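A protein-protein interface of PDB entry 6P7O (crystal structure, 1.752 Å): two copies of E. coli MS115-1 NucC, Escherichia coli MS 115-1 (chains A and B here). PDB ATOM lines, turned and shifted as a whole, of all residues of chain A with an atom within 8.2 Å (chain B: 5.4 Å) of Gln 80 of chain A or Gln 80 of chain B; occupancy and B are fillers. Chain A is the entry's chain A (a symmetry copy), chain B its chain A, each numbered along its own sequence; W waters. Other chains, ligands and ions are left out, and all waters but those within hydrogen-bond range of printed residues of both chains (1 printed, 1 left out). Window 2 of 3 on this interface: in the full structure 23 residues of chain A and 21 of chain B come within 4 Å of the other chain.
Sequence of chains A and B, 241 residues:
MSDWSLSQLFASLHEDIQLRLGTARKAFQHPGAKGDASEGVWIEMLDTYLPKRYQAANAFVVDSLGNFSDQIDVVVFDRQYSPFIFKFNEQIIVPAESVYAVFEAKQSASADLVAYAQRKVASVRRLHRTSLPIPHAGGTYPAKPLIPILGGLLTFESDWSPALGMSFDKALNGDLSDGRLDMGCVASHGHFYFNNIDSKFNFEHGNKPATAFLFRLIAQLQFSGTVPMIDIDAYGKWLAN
The backbone NH of Lys 52 of chain B is in hydrogen-bond range of the backbone carbonyl oxygen of Gln 80 of chain A (3.4 Å). The backbone carbonyl oxygen of Gln 80 of chain A is in hydrogen-bond range of the backbone NH of Arg 53 of chain B.
O of Lys 52 of chain B sits at hydrogen-bond distance from NE of Arg 79 of chain B. The backbone carbonyl oxygen of Arg 53 of chain B lies within hydrogen-bond range of the backbone NH of Arg 79 of chain B. O of Lys 52 of chain A sits at hydrogen-bond distance from NE of Arg 79 of chain A (2.9 Å). O of Tyr 54 of chain A sits at hydrogen-bond distance from NH2 of Arg 79 of chain A, at 2.9 Å. The side-chain carboxylate of Asp 78 of chain A is in hydrogen-bond range of the backbone NH of Tyr 81 of chain A, 2.8 Å away. O of Asp 78 of chain A lies within hydrogen-bond range of OG of Ser 82 of chain A (2.6 Å).
Gln 80 of chain A touches four residues of chain B. Gln 80 of chain B touches just one residue of chain A: Gln 80. Printed residues of chain B within 4 Å of Ser 82 of chain A: Pro 51. Of the printed residues of chain A, Arg 53 of chain B touches Gln 80 (3.1 Å) and Tyr 81 (3.5 Å). Val 227 of chain A touches none of the printed residues of chain B. The nearest residue of chain B that does not touch Gln 80 of chain A is Arg 79 of chain B (4.9 Å). The nearest residue of chain A that does not touch Gln 80 of chain B is Tyr 81 of chain A (6.2 Å). The nearest printed residue of chain A that does not touch Arg 53 of chain B is Arg 79 of chain A (5.9 Å).
Arg 79 of chain A touches Lys 52 of chain B, but with the chains exchanged Lys 52 of chain A does not touch Arg 79 of chain B (10.8 Å). Gln 80 of chain A touches Lys 52 of chain B, but with the chains exchanged Lys 52 of chain A does not touch Gln 80 of chain B (7.6 Å). Gln 80 of chain A touches Arg 53 of chain B, but with the chains exchanged Arg 53 of chain A does not touch Gln 80 of chain B (8.2 Å). Gln 80 of chain A touches its own counterpart, Gln 80 of chain B. Positions printed for both chains: 52, 53, 78, 79, 80, 81 and 82.
Water W1 lies within hydrogen-bond range of OH of Tyr 81 of chain B (3.4 Å) and OH of Tyr 81 of chain A (3.4 Å).
Arg 79 of chain A touches Lys 52 of chain B. CB of Pro 51 of chain B touches O of Gln 80 of chain A (3.6 Å). Gln 80 of chain B touches Gln 80 of chain A (CG to OE1, 3.7 Å). CE2 of Tyr 81 of chain A touches CD of Arg 53 of chain B, 3.5 Å away. Pro 51 of chain B touches Ser 82 of chain A (CB to O, 3.6 Å). CA of Pro 83 of chain A touches CG of Pro 51 of chain B, 3.9 Å away.
Hydrophobic or aromatic side chains of chain A within 4 Å of the printed part of chain B: Tyr 81. Of the 8 printed residues of chain B, 4 touch a printed residue of chain A. Hydrophobic or aromatic side chains of chain B that line the printed part of chain A: Pro 51. Among the printed residues, 8 pairs touch across the chains.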
ATOM      1  N   LYS A  52      25.421  11.305  -2.387  1.00  0.00           N
ATOM      2  CA  LYS A  52      24.091  11.504  -1.844  1.00  0.00           C
ATOM      3  C   LYS A  52      23.177  10.355  -2.190  1.00  0.00           C
ATOM      4  O   LYS A  52      22.097  10.261  -1.635  1.00  0.00           O
ATOM      5  CB  LYS A  52      23.491  12.826  -2.359  1.00  0.00           C
ATOM      6  CG  LYS A  52      24.361  14.055  -2.047  1.00  0.00           C
ATOM      7  CD  LYS A  52      24.928  14.039  -0.629  1.00  0.00           C
ATOM      8  CE  LYS A  52      23.828  13.892   0.422  1.00  0.00           C
ATOM      9  NZ  LYS A  52      24.389  13.752   1.804  1.00  0.00           N
ATOM     10  N   ARG A  53      23.562   9.475  -3.090  1.00  0.00           N
ATOM     11  CA  ARG A  53      22.724   8.297  -3.305  1.00  0.00           C
ATOM     12  C   ARG A  53      22.663   7.422  -2.070  1.00  0.00           C
ATOM     13  O   ARG A  53      21.783   6.541  -1.966  1.00  0.00           O
ATOM     14  CB  ARG A  53      23.217   7.440  -4.461  1.00  0.00           C
ATOM     15  CG  ARG A  53      24.556   6.876  -4.237  1.00  0.00           C
ATOM     16  CD  ARG A  53      24.971   6.052  -5.505  1.00  0.00           C
ATOM     17  NE  ARG A  53      24.258   4.753  -5.522  1.00  0.00           N
ATOM     18  CZ  ARG A  53      24.679   3.673  -6.175  1.00  0.00           C
ATOM     19  NH1 ARG A  53      25.786   3.757  -6.926  1.00  0.00           N
ATOM     20  NH2 ARG A  53      24.000   2.534  -6.099  1.00  0.00           N
ATOM     21  N   TYR A  54      23.617   7.576  -1.169  1.00  0.00           N
ATOM     22  CA  TYR A  54      23.659   6.804   0.079  1.00  0.00           C
ATOM     23  C   TYR A  54      23.178   7.643   1.244  1.00  0.00           C
ATOM     24  O   TYR A  54      23.293   8.867   1.254  1.00  0.00           O
ATOM     25  CB  TYR A  54      25.081   6.292   0.451  1.00  0.00           C
ATOM     26  CG  TYR A  54      25.711   5.527  -0.685  1.00  0.00           C
ATOM     27  CD1 TYR A  54      25.244   4.283  -1.052  1.00  0.00           C
ATOM     28  CD2 TYR A  54      26.767   6.060  -1.395  1.00  0.00           C
ATOM     29  CE1 TYR A  54      25.788   3.600  -2.122  1.00  0.00           C
ATOM     30  CE2 TYR A  54      27.328   5.360  -2.553  1.00  0.00           C
ATOM     31  CZ  TYR A  54      26.776   4.138  -2.854  1.00  0.00           C
ATOM     32  OH  TYR A  54      27.257   3.505  -3.951  1.00  0.00           O
ATOM     33  N   GLN A  55      22.745   6.953   2.277  1.00  0.00           N
ATOM     34  CA  GLN A  55      22.277   7.547   3.517  1.00  0.00           C
ATOM     35  C   GLN A  55      22.891   6.697   4.632  1.00  0.00           C
ATOM     36  O   GLN A  55      23.071   5.468   4.467  1.00  0.00           O
ATOM     37  CB  GLN A  55      20.755   7.506   3.635  1.00  0.00           C
ATOM     38  CG  GLN A  55      20.218   8.188   4.832  1.00  0.00           C
ATOM     39  CD  GLN A  55      18.716   8.491   4.709  1.00  0.00           C
ATOM     40  OE1 GLN A  55      18.052   8.034   3.782  1.00  0.00           O
ATOM     41  NE2 GLN A  55      18.198   9.247   5.630  1.00  0.00           N
ATOM     42  N   PHE A  77      22.754   2.777   3.581  1.00  0.00           N
ATOM     43  CA  PHE A  77      21.663   2.174   2.810  1.00  0.00           C
ATOM     44  C   PHE A  77      21.278   3.108   1.680  1.00  0.00           C
ATOM     45  O   PHE A  77      21.748   4.237   1.583  1.00  0.00           O
ATOM     46  CB  PHE A  77      20.447   1.814   3.756  1.00  0.00           C
ATOM     47  CG  PHE A  77      19.892   2.959   4.535  1.00  0.00           C
ATOM     48  CD1 PHE A  77      20.471   3.355   5.728  1.00  0.00           C
ATOM     49  CD2 PHE A  77      18.812   3.661   4.082  1.00  0.00           C
ATOM     50  CE1 PHE A  77      19.965   4.445   6.454  1.00  0.00           C
ATOM     51  CE2 PHE A  77      18.296   4.730   4.781  1.00  0.00           C
ATOM     52  CZ  PHE A  77      18.889   5.129   5.990  1.00  0.00           C
ATOM     53  N   ASP A  78      20.409   2.616   0.777  1.00  0.00           N
ATOM     54  CA  ASP A  78      20.024   3.392  -0.388  1.00  0.00           C
ATOM     55  C   ASP A  78      19.045   4.496  -0.026  1.00  0.00           C
ATOM     56  O   ASP A  78      17.919   4.228   0.401  1.00  0.00           O
ATOM     57  CB  ASP A  78      19.435   2.440  -1.435  1.00  0.00           C
ATOM     58  CG  ASP A  78      19.368   3.078  -2.755  1.00  0.00           C
ATOM     59  OD1 ASP A  78      18.670   4.090  -2.905  1.00  0.00           O
ATOM     60  OD2 ASP A  78      20.093   2.707  -3.627  1.00  0.00           O
ATOM     61  N   ARG A  79      19.389   5.716  -0.365  1.00  0.00           N
ATOM     62  CA  ARG A  79      18.561   6.847   0.022  1.00  0.00           C
ATOM     63  C   ARG A  79      17.259   6.907  -0.752  1.00  0.00           C
ATOM     64  O   ARG A  79      16.195   7.202  -0.170  1.00  0.00           O
ATOM     65  CB  ARG A  79      19.337   8.156  -0.179  1.00  0.00           C
ATOM     66  CG  ARG A  79      18.626   9.428   0.399  1.00  0.00           C
ATOM     67  CD  ARG A  79      19.418  10.680   0.191  1.00  0.00           C
ATOM     68  NE  ARG A  79      20.694  10.666   0.921  1.00  0.00           N
ATOM     69  CZ  ARG A  79      20.852  11.036   2.186  1.00  0.00           C
ATOM     70  NH1 ARG A  79      19.830  11.403   2.908  1.00  0.00           N
ATOM     71  NH2 ARG A  79      22.033  11.028   2.729  1.00  0.00           N
ATOM     72  N   GLN A  80      17.314   6.749  -2.078  1.00  0.00           N
ATOM     73  CA  GLN A  80      16.161   7.064  -2.936  1.00  0.00           C
ATOM     74  C   GLN A  80      15.326   5.858  -3.286  1.00  0.00           C
ATOM     75  O   GLN A  80      14.205   6.034  -3.782  1.00  0.00           O
ATOM     76  CB  GLN A  80      16.605   7.686  -4.285  1.00  0.00           C
ATOM     77  CG  GLN A  80      17.516   8.841  -4.237  1.00  0.00           C
ATOM     78  CD  GLN A  80      16.772  10.059  -3.989  1.00  0.00           C
ATOM     79  OE1 GLN A  80      16.104  10.604  -4.887  1.00  0.00           O
ATOM     80  NE2 GLN A  80      16.813  10.496  -2.753  1.00  0.00           N
ATOM     81  N   TYR A  81      15.946   4.690  -3.254  1.00  0.00           N
ATOM     82  CA  TYR A  81      15.328   3.468  -3.761  1.00  0.00           C
ATOM     83  C   TYR A  81      15.007   2.441  -2.648  1.00  0.00           C
ATOM     84  O   TYR A  81      14.520   1.350  -2.954  1.00  0.00           O
ATOM     85  CB  TYR A  81      16.234   2.789  -4.824  1.00  0.00           C
ATOM     86  CG  TYR A  81      16.484   3.668  -6.020  1.00  0.00           C
ATOM     87  CD1 TYR A  81      17.476   4.623  -6.005  1.00  0.00           C
ATOM     88  CD2 TYR A  81      15.661   3.584  -7.148  1.00  0.00           C
ATOM     89  CE1 TYR A  81      17.651   5.484  -7.065  1.00  0.00           C
ATOM     90  CE2 TYR A  81      15.842   4.427  -8.240  1.00  0.00           C
ATOM     91  CZ  TYR A  81      16.819   5.396  -8.177  1.00  0.00           C
ATOM     92  OH  TYR A  81      17.062   6.281  -9.219  1.00  0.00           O
ATOM     93  N   SER A  82      15.225   2.783  -1.382  1.00  0.00           N
ATOM     94  CA  SER A  82      14.745   1.887  -0.322  1.00  0.00           C
ATOM     95  C   SER A  82      13.210   1.954  -0.338  1.00  0.00           C
ATOM     96  O   SER A  82      12.637   3.042  -0.385  1.00  0.00           O
ATOM     97  CB  SER A  82      15.235   2.246   1.066  1.00  0.00           C
ATOM     98  OG  SER A  82      16.645   2.137   1.233  1.00  0.00           O
ATOM     99  N   PRO A  83      12.527   0.823  -0.226  1.00  0.00           N
ATOM    100  CA  PRO A  83      11.057   0.828  -0.297  1.00  0.00           C
ATOM    101  C   PRO A  83      10.402   1.361   0.978  1.00  0.00           C
ATOM    102  O   PRO A  83       9.306   1.916   0.924  1.00  0.00           O
ATOM    103  CB  PRO A  83      10.703  -0.662  -0.507  1.00  0.00           C
ATOM    104  CG  PRO A  83      11.872  -1.405   0.212  1.00  0.00           C
ATOM    105  CD  PRO A  83      13.091  -0.519  -0.109  1.00  0.00           C
ATOM    106  N   SER A  98      18.311  -3.181   0.992  1.00  0.00           N
ATOM    107  CA  SER A  98      18.736  -1.856   0.573  1.00  0.00           C
ATOM    108  C   SER A  98      19.978  -1.419   1.347  1.00  0.00           C
ATOM    109  O   SER A  98      20.418  -0.274   1.199  1.00  0.00           O
ATOM    110  CB  SER A  98      17.521  -0.911   0.673  1.00  0.00           C
ATOM    111  OG  SER A  98      17.232  -0.567   1.944  1.00  0.00           O
ATOM    112  N   TYR A 100      24.019  -1.352   2.053  1.00  0.00           N
ATOM    113  CA  TYR A 100      25.314  -1.461   1.384  1.00  0.00           C
ATOM    114  C   TYR A 100      26.470  -1.732   2.320  1.00  0.00           C
ATOM    115  O   TYR A 100      27.441  -2.348   1.881  1.00  0.00           O
ATOM    116  CB  TYR A 100      25.650  -0.171   0.621  1.00  0.00           C
ATOM    117  CG  TYR A 100      24.773   0.162  -0.534  1.00  0.00           C
ATOM    118  CD1 TYR A 100      25.103  -0.340  -1.789  1.00  0.00           C
ATOM    119  CD2 TYR A 100      23.724   1.044  -0.444  1.00  0.00           C
ATOM    120  CE1 TYR A 100      24.347  -0.057  -2.923  1.00  0.00           C
ATOM    121  CE2 TYR A 100      22.978   1.343  -1.631  1.00  0.00           C
ATOM    122  CZ  TYR A 100      23.284   0.773  -2.803  1.00  0.00           C
ATOM    123  OH  TYR A 100      22.530   1.037  -3.941  1.00  0.00           O
ATOM    124  N   VAL A 227      19.794  -1.622  -5.638  1.00  0.00           N
ATOM    125  CA  VAL A 227      18.831  -2.400  -4.854  1.00  0.00           C
ATOM    126  C   VAL A 227      18.124  -3.345  -5.801  1.00  0.00           C
ATOM    127  O   VAL A 227      17.681  -2.913  -6.857  1.00  0.00           O
ATOM    128  CB  VAL A 227      17.851  -1.455  -4.176  1.00  0.00           C
ATOM    129  CG1 VAL A 227      16.754  -2.169  -3.394  1.00  0.00           C
ATOM    130  CG2 VAL A 227      18.612  -0.532  -3.164  1.00  0.00           C
ATOM    131  N   PRO B  51       9.114   5.908  -1.641  1.00  0.00           N
ATOM    132  CA  PRO B  51      10.552   6.079  -1.896  1.00  0.00           C
ATOM    133  C   PRO B  51      10.810   7.442  -2.520  1.00  0.00           C
ATOM    134  O   PRO B  51      10.024   7.925  -3.332  1.00  0.00           O
ATOM    135  CB  PRO B  51      10.878   4.933  -2.873  1.00  0.00           C
ATOM    136  CG  PRO B  51       9.835   3.849  -2.511  1.00  0.00           C
ATOM    137  CD  PRO B  51       8.568   4.649  -2.189  1.00  0.00           C
ATOM    138  N   LYS B  52      11.969   8.019  -2.128  1.00  0.00           N
ATOM    139  CA  LYS B  52      12.238   9.405  -2.457  1.00  0.00           C
ATOM    140  C   LYS B  52      12.455   9.588  -3.938  1.00  0.00           C
ATOM    141  O   LYS B  52      12.478  10.712  -4.406  1.00  0.00           O
ATOM    142  CB  LYS B  52      13.466   9.916  -1.679  1.00  0.00           C
ATOM    143  CG  LYS B  52      13.328   9.769  -0.155  1.00  0.00           C
ATOM    144  CD  LYS B  52      11.947  10.167   0.360  1.00  0.00           C
ATOM    145  CE  LYS B  52      11.567  11.585  -0.068  1.00  0.00           C
ATOM    146  NZ  LYS B  52      10.165  11.933   0.329  1.00  0.00           N
ATOM    147  N   ARG B  53      12.620   8.527  -4.700  1.00  0.00           N
ATOM    148  CA  ARG B  53      12.688   8.720  -6.148  1.00  0.00           C
ATOM    149  C   ARG B  53      11.385   9.258  -6.700  1.00  0.00           C
ATOM    150  O   ARG B  53      11.344   9.751  -7.847  1.00  0.00           O
ATOM    151  CB  ARG B  53      13.015   7.432  -6.888  1.00  0.00           C
ATOM    152  CG  ARG B  53      11.988   6.393  -6.725  1.00  0.00           C
ATOM    153  CD  ARG B  53      12.452   5.107  -7.495  1.00  0.00           C
ATOM    154  NE  ARG B  53      12.257   5.289  -8.952  1.00  0.00           N
ATOM    155  CZ  ARG B  53      12.129   4.292  -9.824  1.00  0.00           C
ATOM    156  NH1 ARG B  53      12.244   3.029  -9.390  1.00  0.00           N
ATOM    157  NH2 ARG B  53      11.911   4.547 -11.110  1.00  0.00           N
ATOM    158  N   ASP B  78       8.199  11.354 -11.363  1.00  0.00           N
ATOM    159  CA  ASP B  78       9.613  11.171 -11.086  1.00  0.00           C
ATOM    160  C   ASP B  78      10.235  12.428 -10.503  1.00  0.00           C
ATOM    161  O   ASP B  78      10.308  13.465 -11.168  1.00  0.00           O
ATOM    162  CB  ASP B  78      10.312  10.746 -12.382  1.00  0.00           C
ATOM    163  CG  ASP B  78      11.644  10.191 -12.109  1.00  0.00           C
ATOM    164  OD1 ASP B  78      12.501  10.908 -11.576  1.00  0.00           O
ATOM    165  OD2 ASP B  78      11.840   9.026 -12.268  1.00  0.00           O
ATOM    166  N   ARG B  79      10.848  12.296  -9.350  1.00  0.00           N
ATOM    167  CA  ARG B  79      11.393  13.459  -8.670  1.00  0.00           C
ATOM    168  C   ARG B  79      12.626  14.011  -9.359  1.00  0.00           C
ATOM    169  O   ARG B  79      12.780  15.244  -9.476  1.00  0.00           O
ATOM    170  CB  ARG B  79      11.735  13.103  -7.217  1.00  0.00           C
ATOM    171  CG  ARG B  79      12.135  14.328  -6.324  1.00  0.00           C
ATOM    172  CD  ARG B  79      12.451  13.941  -4.914  1.00  0.00           C
ATOM    173  NE  ARG B  79      11.285  13.395  -4.206  1.00  0.00           N
ATOM    174  CZ  ARG B  79      10.371  14.120  -3.571  1.00  0.00           C
ATOM    175  NH1 ARG B  79      10.427  15.423  -3.580  1.00  0.00           N
ATOM    176  NH2 ARG B  79       9.397  13.537  -2.937  1.00  0.00           N
ATOM    177  N   GLN B  80      13.576  13.146  -9.724  1.00  0.00           N
ATOM    178  CA  GLN B  80      14.911  13.604 -10.139  1.00  0.00           C
ATOM    179  C   GLN B  80      15.073  13.708 -11.634  1.00  0.00           C
ATOM    180  O   GLN B  80      16.051  14.318 -12.087  1.00  0.00           O
ATOM    181  CB  GLN B  80      16.023  12.639  -9.653  1.00  0.00           C
ATOM    182  CG  GLN B  80      16.044  12.286  -8.224  1.00  0.00           C
ATOM    183  CD  GLN B  80      16.696  13.327  -7.457  1.00  0.00           C
ATOM    184  OE1 GLN B  80      17.934  13.454  -7.459  1.00  0.00           O
ATOM    185  NE2 GLN B  80      15.887  14.141  -6.823  1.00  0.00           N
ATOM    186  N   TYR B  81      14.279  12.940 -12.362  1.00  0.00           N
ATOM    187  CA  TYR B  81      14.456  12.782 -13.803  1.00  0.00           C
ATOM    188  C   TYR B  81      13.305  13.405 -14.629  1.00  0.00           C
ATOM    189  O   TYR B  81      13.318  13.301 -15.858  1.00  0.00           O
ATOM    190  CB  TYR B  81      14.593  11.282 -14.183  1.00  0.00           C
ATOM    191  CG  TYR B  81      15.780  10.624 -13.533  1.00  0.00           C
ATOM    192  CD1 TYR B  81      15.706  10.136 -12.247  1.00  0.00           C
ATOM    193  CD2 TYR B  81      17.010  10.564 -14.196  1.00  0.00           C
ATOM    194  CE1 TYR B  81      16.815   9.610 -11.621  1.00  0.00           C
ATOM    195  CE2 TYR B  81      18.133  10.011 -13.589  1.00  0.00           C
ATOM    196  CZ  TYR B  81      18.035   9.565 -12.289  1.00  0.00           C
ATOM    197  OH  TYR B  81      19.107   9.006 -11.607  1.00  0.00           O
ATOM    198  N   SER B  82      12.352  14.077 -13.992  1.00  0.00           N
ATOM    199  CA  SER B  82      11.371  14.825 -14.787  1.00  0.00           C
ATOM    200  C   SER B  82      12.117  16.003 -15.431  1.00  0.00           C
ATOM    201  O   SER B  82      12.868  16.705 -14.755  1.00  0.00           O
ATOM    202  CB  SER B  82      10.202  15.366 -13.986  1.00  0.00           C
ATOM    203  OG  SER B  82       9.377  14.360 -13.408  1.00  0.00           O
HETATM  204  O   HOH W   1      18.721   9.084  -8.224  1.00  0.00           O
